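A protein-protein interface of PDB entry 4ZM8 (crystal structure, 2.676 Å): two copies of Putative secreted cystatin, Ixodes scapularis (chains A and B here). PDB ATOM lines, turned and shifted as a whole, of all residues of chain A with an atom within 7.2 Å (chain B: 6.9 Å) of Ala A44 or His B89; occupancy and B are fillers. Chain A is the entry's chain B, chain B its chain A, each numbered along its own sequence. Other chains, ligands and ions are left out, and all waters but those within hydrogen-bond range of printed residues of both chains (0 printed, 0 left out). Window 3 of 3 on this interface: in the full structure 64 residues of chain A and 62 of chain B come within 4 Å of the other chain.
The backbone carbonyl oxygen (O) of Lys B64 sits at hydrogen-bond distance from the backbone NH (N) of Ala A44 (2.7 Å).
The backbone carbonyl oxygen of Glu A45 is in hydrogen-bond range of the backbone NH of Lys B64.
The backbone NH (N) of Thr A42 lies within hydrogen-bond range of the backbone carbonyl oxygen (O) of Ala B66.
The backbone carbonyl oxygen (O) of Arg B90 lies within hydrogen-bond range of the backbone NH (N) of Val B65, 2.8 Å away.
The backbone carbonyl oxygen of Ala B87 lies within hydrogen-bond range of a ring nitrogen (ND1) of His B89, 3.1 Å away.
Among the printed residues, pairs that only touch across the chains: Glu A45 with Leu B63 (3.4 Å), Thr A42 with Val B65 (3.4 Å), Thr A42 with Pro B83 (3.6 Å), Thr A27 with Leu B63 (3.6 Å), Val A43 with Lys B64 (3.7 Å), Val A46 with Leu B63 (3.9 Å), Ala A44 with His B89 (3.9 Å) and Thr A42 with Lys B64 (3.98 Å).
Printed residues of chain B within 4 Å of Thr A42: Lys B64, Val B65, Ala B66 and Pro B83.
Of chain B, only Lys B64 (2.7 Å) and His B89 (3.9 Å) come within 4 Å of Ala A44.
Of the printed residues of chain B, Val A46 touches Leu B63.
Printed residues of chain A within 4 Å of Lys B64: Thr A42 (3.98 Å), Val A43 (3.7 Å), Ala A44 (2.7 Å) and Glu A45 (2.7 Å).
Of chain A, only Ala A44 comes within 4 Å of His B89.
The nearest residue of chain B that does not touch Ala A44 is Val B65 (4.4 Å).
Of the 15 printed residues of chain B, 6 touch a printed residue of chain A.
Hydrophobic or aromatic side chains of chain B that line the printed part of chain A: Leu B63, Val B65, Pro B83 and His B89.
Of the 8 printed residues of chain A, 6 touch a printed residue of chain B.
Hydrophobic or aromatic side chains of chain A that line the printed part of chain B: Ala A44.
Among the printed residues, no Asp or Glu carboxylate lies within 4 Å of a Lys or Arg side-chain nitrogen of the other chain.
No position is printed for both chains.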
ATOM      1  N   LEU A  20      -3.841  -3.087  -3.333  1.00  0.00           N
ATOM      2  CA  LEU A  20      -4.152  -2.297  -2.144  1.00  0.00           C
ATOM      3  C   LEU A  20      -5.667  -2.199  -1.995  1.00  0.00           C
ATOM      4  O   LEU A  20      -6.229  -2.603  -0.978  1.00  0.00           O
ATOM      5  CB  LEU A  20      -3.509  -0.909  -2.215  1.00  0.00           C
ATOM      6  CG  LEU A  20      -3.735   0.066  -1.044  1.00  0.00           C
ATOM      7  CD1 LEU A  20      -3.088  -0.424   0.246  1.00  0.00           C
ATOM      8  CD2 LEU A  20      -3.245   1.490  -1.366  1.00  0.00           C
ATOM      9  N   HIS A  24      -8.012  -3.411   1.279  1.00  0.00           N
ATOM     10  CA  HIS A  24      -8.969  -2.583   1.998  1.00  0.00           C
ATOM     11  C   HIS A  24     -10.353  -3.237   2.007  1.00  0.00           C
ATOM     12  O   HIS A  24     -10.986  -3.352   3.059  1.00  0.00           O
ATOM     13  CB  HIS A  24      -9.044  -1.181   1.383  1.00  0.00           C
ATOM     14  CG  HIS A  24      -7.956  -0.261   1.834  1.00  0.00           C
ATOM     15  ND1 HIS A  24      -7.779   0.089   3.155  1.00  0.00           N
ATOM     16  CD2 HIS A  24      -6.990   0.385   1.141  1.00  0.00           C
ATOM     17  CE1 HIS A  24      -6.749   0.910   3.257  1.00  0.00           C
ATOM     18  NE2 HIS A  24      -6.255   1.106   2.048  1.00  0.00           N
ATOM     19  N   THR A  27     -10.456  -6.117   4.410  1.00  0.00           N
ATOM     20  CA  THR A  27     -10.265  -5.796   5.822  1.00  0.00           C
ATOM     21  C   THR A  27     -11.495  -5.125   6.414  1.00  0.00           C
ATOM     22  O   THR A  27     -11.893  -5.419   7.542  1.00  0.00           O
ATOM     23  CB  THR A  27      -9.037  -4.892   6.017  1.00  0.00           C
ATOM     24  OG1 THR A  27      -7.906  -5.501   5.390  1.00  0.00           O
ATOM     25  CG2 THR A  27      -8.752  -4.656   7.488  1.00  0.00           C
ATOM     26  N   THR A  42      -8.427  -1.472   9.460  1.00  0.00           N
ATOM     27  CA  THR A  42      -7.948  -1.019   8.168  1.00  0.00           C
ATOM     28  C   THR A  42      -6.567  -1.550   7.876  1.00  0.00           C
ATOM     29  O   THR A  42      -5.994  -2.298   8.663  1.00  0.00           O
ATOM     30  CB  THR A  42      -7.914   0.515   8.062  1.00  0.00           C
ATOM     31  OG1 THR A  42      -7.693   0.905   6.694  1.00  0.00           O
ATOM     32  CG2 THR A  42      -6.807   1.084   8.938  1.00  0.00           C
ATOM     33  N   VAL A  43      -6.059  -1.171   6.711  1.00  0.00           N
ATOM     34  CA  VAL A  43      -4.747  -1.580   6.264  1.00  0.00           C
ATOM     35  C   VAL A  43      -3.657  -0.652   6.802  1.00  0.00           C
ATOM     36  O   VAL A  43      -3.695   0.563   6.582  1.00  0.00           O
ATOM     37  CB  VAL A  43      -4.680  -1.598   4.738  1.00  0.00           C
ATOM     38  CG1 VAL A  43      -3.273  -1.933   4.277  1.00  0.00           C
ATOM     39  CG2 VAL A  43      -5.700  -2.582   4.185  1.00  0.00           C
ATOM     40  N   ALA A  44      -2.696  -1.224   7.523  1.00  0.00           N
ATOM     41  CA  ALA A  44      -1.507  -0.486   7.924  1.00  0.00           C
ATOM     42  C   ALA A  44      -0.465  -0.686   6.856  1.00  0.00           C
ATOM     43  O   ALA A  44       0.341   0.208   6.587  1.00  0.00           O
ATOM     44  CB  ALA A  44      -0.982  -0.949   9.271  1.00  0.00           C
ATOM     45  N   GLU A  45      -0.498  -1.864   6.236  1.00  0.00           N
ATOM     46  CA  GLU A  45       0.508  -2.228   5.246  1.00  0.00           C
ATOM     47  C   GLU A  45       0.207  -3.535   4.530  1.00  0.00           C
ATOM     48  O   GLU A  45      -0.104  -4.550   5.162  1.00  0.00           O
ATOM     49  CB  GLU A  45       1.897  -2.333   5.908  1.00  0.00           C
ATOM     50  CG  GLU A  45       2.965  -2.946   5.023  1.00  0.00           C
ATOM     51  CD  GLU A  45       4.339  -2.415   5.343  1.00  0.00           C
ATOM     52  OE1 GLU A  45       4.602  -1.217   5.031  1.00  0.00           O
ATOM     53  OE2 GLU A  45       5.144  -3.198   5.916  1.00  0.00           O
ATOM     54  N   VAL A  46       0.328  -3.506   3.209  1.00  0.00           N
ATOM     55  CA  VAL A  46       0.366  -4.728   2.445  1.00  0.00           C
ATOM     56  C   VAL A  46       1.778  -5.302   2.540  1.00  0.00           C
ATOM     57  O   VAL A  46       2.741  -4.681   2.075  1.00  0.00           O
ATOM     58  CB  VAL A  46      -0.018  -4.493   0.987  1.00  0.00           C
ATOM     59  CG1 VAL A  46      -0.119  -5.820   0.240  1.00  0.00           C
ATOM     60  CG2 VAL A  46      -1.332  -3.736   0.915  1.00  0.00           C
ATOM     61  N   LEU B  63      -0.990  -8.953   5.604  1.00  0.00           N
ATOM     62  CA  LEU B  63      -1.331  -7.583   5.953  1.00  0.00           C
ATOM     63  C   LEU B  63      -0.921  -7.190   7.346  1.00  0.00           C
ATOM     64  O   LEU B  63      -0.943  -8.009   8.262  1.00  0.00           O
ATOM     65  CB  LEU B  63      -2.839  -7.357   5.834  1.00  0.00           C
ATOM     66  CG  LEU B  63      -3.464  -7.609   4.478  1.00  0.00           C
ATOM     67  CD1 LEU B  63      -4.939  -7.306   4.563  1.00  0.00           C
ATOM     68  CD2 LEU B  63      -2.763  -6.757   3.432  1.00  0.00           C
ATOM     69  N   LYS B  64      -0.576  -5.918   7.492  1.00  0.00           N
ATOM     70  CA  LYS B  64      -0.547  -5.269   8.795  1.00  0.00           C
ATOM     71  C   LYS B  64      -1.907  -4.608   9.004  1.00  0.00           C
ATOM     72  O   LYS B  64      -2.334  -3.789   8.193  1.00  0.00           O
ATOM     73  CB  LYS B  64       0.577  -4.233   8.877  1.00  0.00           C
ATOM     74  CG  LYS B  64       1.974  -4.802   8.888  1.00  0.00           C
ATOM     75  CD  LYS B  64       2.251  -5.535  10.183  1.00  0.00           C
ATOM     76  CE  LYS B  64       3.633  -6.171  10.157  1.00  0.00           C
ATOM     77  NZ  LYS B  64       4.680  -5.221   9.644  1.00  0.00           N
ATOM     78  N   VAL B  65      -2.588  -4.972  10.081  1.00  0.00           N
ATOM     79  CA  VAL B  65      -3.941  -4.496  10.332  1.00  0.00           C
ATOM     80  C   VAL B  65      -3.989  -3.609  11.585  1.00  0.00           C
ATOM     81  O   VAL B  65      -3.277  -3.852  12.553  1.00  0.00           O
ATOM     82  CB  VAL B  65      -4.897  -5.704  10.457  1.00  0.00           C
ATOM     83  CG1 VAL B  65      -6.300  -5.273  10.805  1.00  0.00           C
ATOM     84  CG2 VAL B  65      -4.911  -6.456   9.160  1.00  0.00           C
ATOM     85  N   ALA B  66      -4.812  -2.568  11.553  1.00  0.00           N
ATOM     86  CA  ALA B  66      -4.957  -1.658  12.691  1.00  0.00           C
ATOM     87  C   ALA B  66      -6.375  -1.080  12.793  1.00  0.00           C
ATOM     88  O   ALA B  66      -7.021  -0.817  11.765  1.00  0.00           O
ATOM     89  CB  ALA B  66      -3.941  -0.537  12.590  1.00  0.00           C
ATOM     90  N   GLU B  67      -6.851  -0.899  14.032  1.00  0.00           N
ATOM     91  CA  GLU B  67      -8.152  -0.283  14.302  1.00  0.00           C
ATOM     92  C   GLU B  67      -8.197   1.069  13.584  1.00  0.00           C
ATOM     93  O   GLU B  67      -7.216   1.813  13.600  1.00  0.00           O
ATOM     94  CB  GLU B  67      -8.380  -0.141  15.821  1.00  0.00           C
ATOM     95  CG  GLU B  67      -9.755   0.424  16.262  1.00  0.00           C
ATOM     96  CD  GLU B  67     -10.018   0.331  17.781  1.00  0.00           C
ATOM     97  OE1 GLU B  67     -11.082   0.805  18.245  1.00  0.00           O
ATOM     98  OE2 GLU B  67      -9.168  -0.214  18.519  1.00  0.00           O
ATOM     99  N   PRO B  83      -5.529   4.290   9.770  1.00  0.00           N
ATOM    100  CA  PRO B  83      -5.166   3.590  11.002  1.00  0.00           C
ATOM    101  C   PRO B  83      -4.938   4.535  12.181  1.00  0.00           C
ATOM    102  O   PRO B  83      -4.179   5.504  12.061  1.00  0.00           O
ATOM    103  CB  PRO B  83      -3.875   2.856  10.615  1.00  0.00           C
ATOM    104  CG  PRO B  83      -3.374   3.549   9.418  1.00  0.00           C
ATOM    105  CD  PRO B  83      -4.562   4.035   8.692  1.00  0.00           C
ATOM    106  N   LYS B  84      -5.614   4.265  13.294  1.00  0.00           N
ATOM    107  CA  LYS B  84      -5.313   4.927  14.566  1.00  0.00           C
ATOM    108  C   LYS B  84      -3.802   4.893  14.900  1.00  0.00           C
ATOM    109  O   LYS B  84      -3.197   3.824  15.019  1.00  0.00           O
ATOM    110  CB  LYS B  84      -6.093   4.279  15.715  1.00  0.00           C
ATOM    111  CG  LYS B  84      -7.417   4.918  16.051  1.00  0.00           C
ATOM    112  CD  LYS B  84      -7.754   4.740  17.540  1.00  0.00           C
ATOM    113  CE  LYS B  84      -7.876   3.254  17.918  1.00  0.00           C
ATOM    114  NZ  LYS B  84      -8.126   2.986  19.373  1.00  0.00           N
ATOM    115  N   ALA B  85      -3.227   6.085  15.058  1.00  0.00           N
ATOM    116  CA  ALA B  85      -1.841   6.297  15.464  1.00  0.00           C
ATOM    117  C   ALA B  85      -1.318   5.381  16.571  1.00  0.00           C
ATOM    118  O   ALA B  85      -0.166   4.941  16.494  1.00  0.00           O
ATOM    119  CB  ALA B  85      -1.642   7.774  15.894  1.00  0.00           C
ATOM    120  N   ASP B  86      -2.104   5.119  17.616  1.00  0.00           N
ATOM    121  CA  ASP B  86      -1.590   4.257  18.691  1.00  0.00           C
ATOM    122  C   ASP B  86      -2.156   2.830  18.660  1.00  0.00           C
ATOM    123  O   ASP B  86      -1.955   2.053  19.591  1.00  0.00           O
ATOM    124  CB  ASP B  86      -1.826   4.890  20.076  1.00  0.00           C
ATOM    125  CG  ASP B  86      -3.301   5.101  20.411  1.00  0.00           C
ATOM    126  OD1 ASP B  86      -4.120   4.180  20.221  1.00  0.00           O
ATOM    127  OD2 ASP B  86      -3.643   6.206  20.896  1.00  0.00           O
ATOM    128  N   ALA B  87      -2.845   2.472  17.588  1.00  0.00           N
ATOM    129  CA  ALA B  87      -3.402   1.133  17.493  1.00  0.00           C
ATOM    130  C   ALA B  87      -2.311   0.109  17.188  1.00  0.00           C
ATOM    131  O   ALA B  87      -1.477   0.300  16.299  1.00  0.00           O
ATOM    132  CB  ALA B  87      -4.490   1.088  16.445  1.00  0.00           C
ATOM    133  N   ALA B  88      -2.316  -0.973  17.955  1.00  0.00           N
ATOM    134  CA  ALA B  88      -1.412  -2.093  17.719  1.00  0.00           C
ATOM    135  C   ALA B  88      -1.654  -2.709  16.344  1.00  0.00           C
ATOM    136  O   ALA B  88      -2.791  -2.927  15.952  1.00  0.00           O
ATOM    137  CB  ALA B  88      -1.581  -3.140  18.801  1.00  0.00           C
ATOM    138  N   HIS B  89      -0.576  -2.972  15.611  1.00  0.00           N
ATOM    139  CA  HIS B  89      -0.658  -3.615  14.307  1.00  0.00           C
ATOM    140  C   HIS B  89      -0.659  -5.142  14.468  1.00  0.00           C
ATOM    141  O   HIS B  89       0.045  -5.673  15.329  1.00  0.00           O
ATOM    142  CB  HIS B  89       0.517  -3.186  13.419  1.00  0.00           C
ATOM    143  CG  HIS B  89       0.573  -1.711  13.127  1.00  0.00           C
ATOM    144  ND1 HIS B  89      -0.348  -0.806  13.612  1.00  0.00           N
ATOM    145  CD2 HIS B  89       1.440  -0.990  12.377  1.00  0.00           C
ATOM    146  CE1 HIS B  89      -0.052   0.403  13.171  1.00  0.00           C
ATOM    147  NE2 HIS B  89       1.028   0.318  12.420  1.00  0.00           N
ATOM    148  N   ARG B  90      -1.442  -5.851  13.657  1.00  0.00           N
ATOM    149  CA  ARG B  90      -1.360  -7.310  13.643  1.00  0.00           C
ATOM    150  C   ARG B  90      -1.060  -7.831  12.239  1.00  0.00           C
ATOM    151  O   ARG B  90      -1.535  -7.293  11.240  1.00  0.00           O
ATOM    152  CB  ARG B  90      -2.651  -7.939  14.149  1.00  0.00           C
ATOM    153  CG  ARG B  90      -3.493  -6.996  14.926  1.00  0.00           C
ATOM    154  CD  ARG B  90      -4.936  -7.266  14.617  1.00  0.00           C
ATOM    155  NE  ARG B  90      -5.749  -6.122  14.973  1.00  0.00           N
ATOM    156  CZ  ARG B  90      -7.031  -6.008  14.660  1.00  0.00           C
ATOM    157  NH1 ARG B  90      -7.637  -6.992  14.003  1.00  0.00           N
ATOM    158  NH2 ARG B  90      -7.703  -4.914  15.023  1.00  0.00           N
ATOM    159  N   THR B  91      -0.258  -8.884  12.170  1.00  0.00           N
ATOM    160  CA  THR B  91       0.025  -9.524  10.898  1.00  0.00           C
ATOM    161  C   THR B  91      -1.025 -10.602  10.643  1.00  0.00           C
ATOM    162  O   THR B  91      -1.163 -11.540  11.426  1.00  0.00           O
ATOM    163  CB  THR B  91       1.448 -10.114  10.875  1.00  0.00           C
ATOM    164  OG1 THR B  91       2.398  -9.052  11.039  1.00  0.00           O
ATOM    165  CG2 THR B  91       1.711 -10.788   9.560  1.00  0.00           C
ATOM    166  N   ALA B 114       1.416 -13.662  18.030  1.00  0.00           N
ATOM    167  CA  ALA B 114       2.502 -12.822  18.548  1.00  0.00           C
ATOM    168  C   ALA B 114       2.055 -11.417  18.974  1.00  0.00           C
ATOM    169  O   ALA B 114       2.607 -10.845  19.918  1.00  0.00           O
ATOM    170  CB  ALA B 114       3.618 -12.716  17.505  1.00  0.00           C
ATOM    171  OXT ALA B 114       1.140 -10.821  18.396  1.00  0.00           O
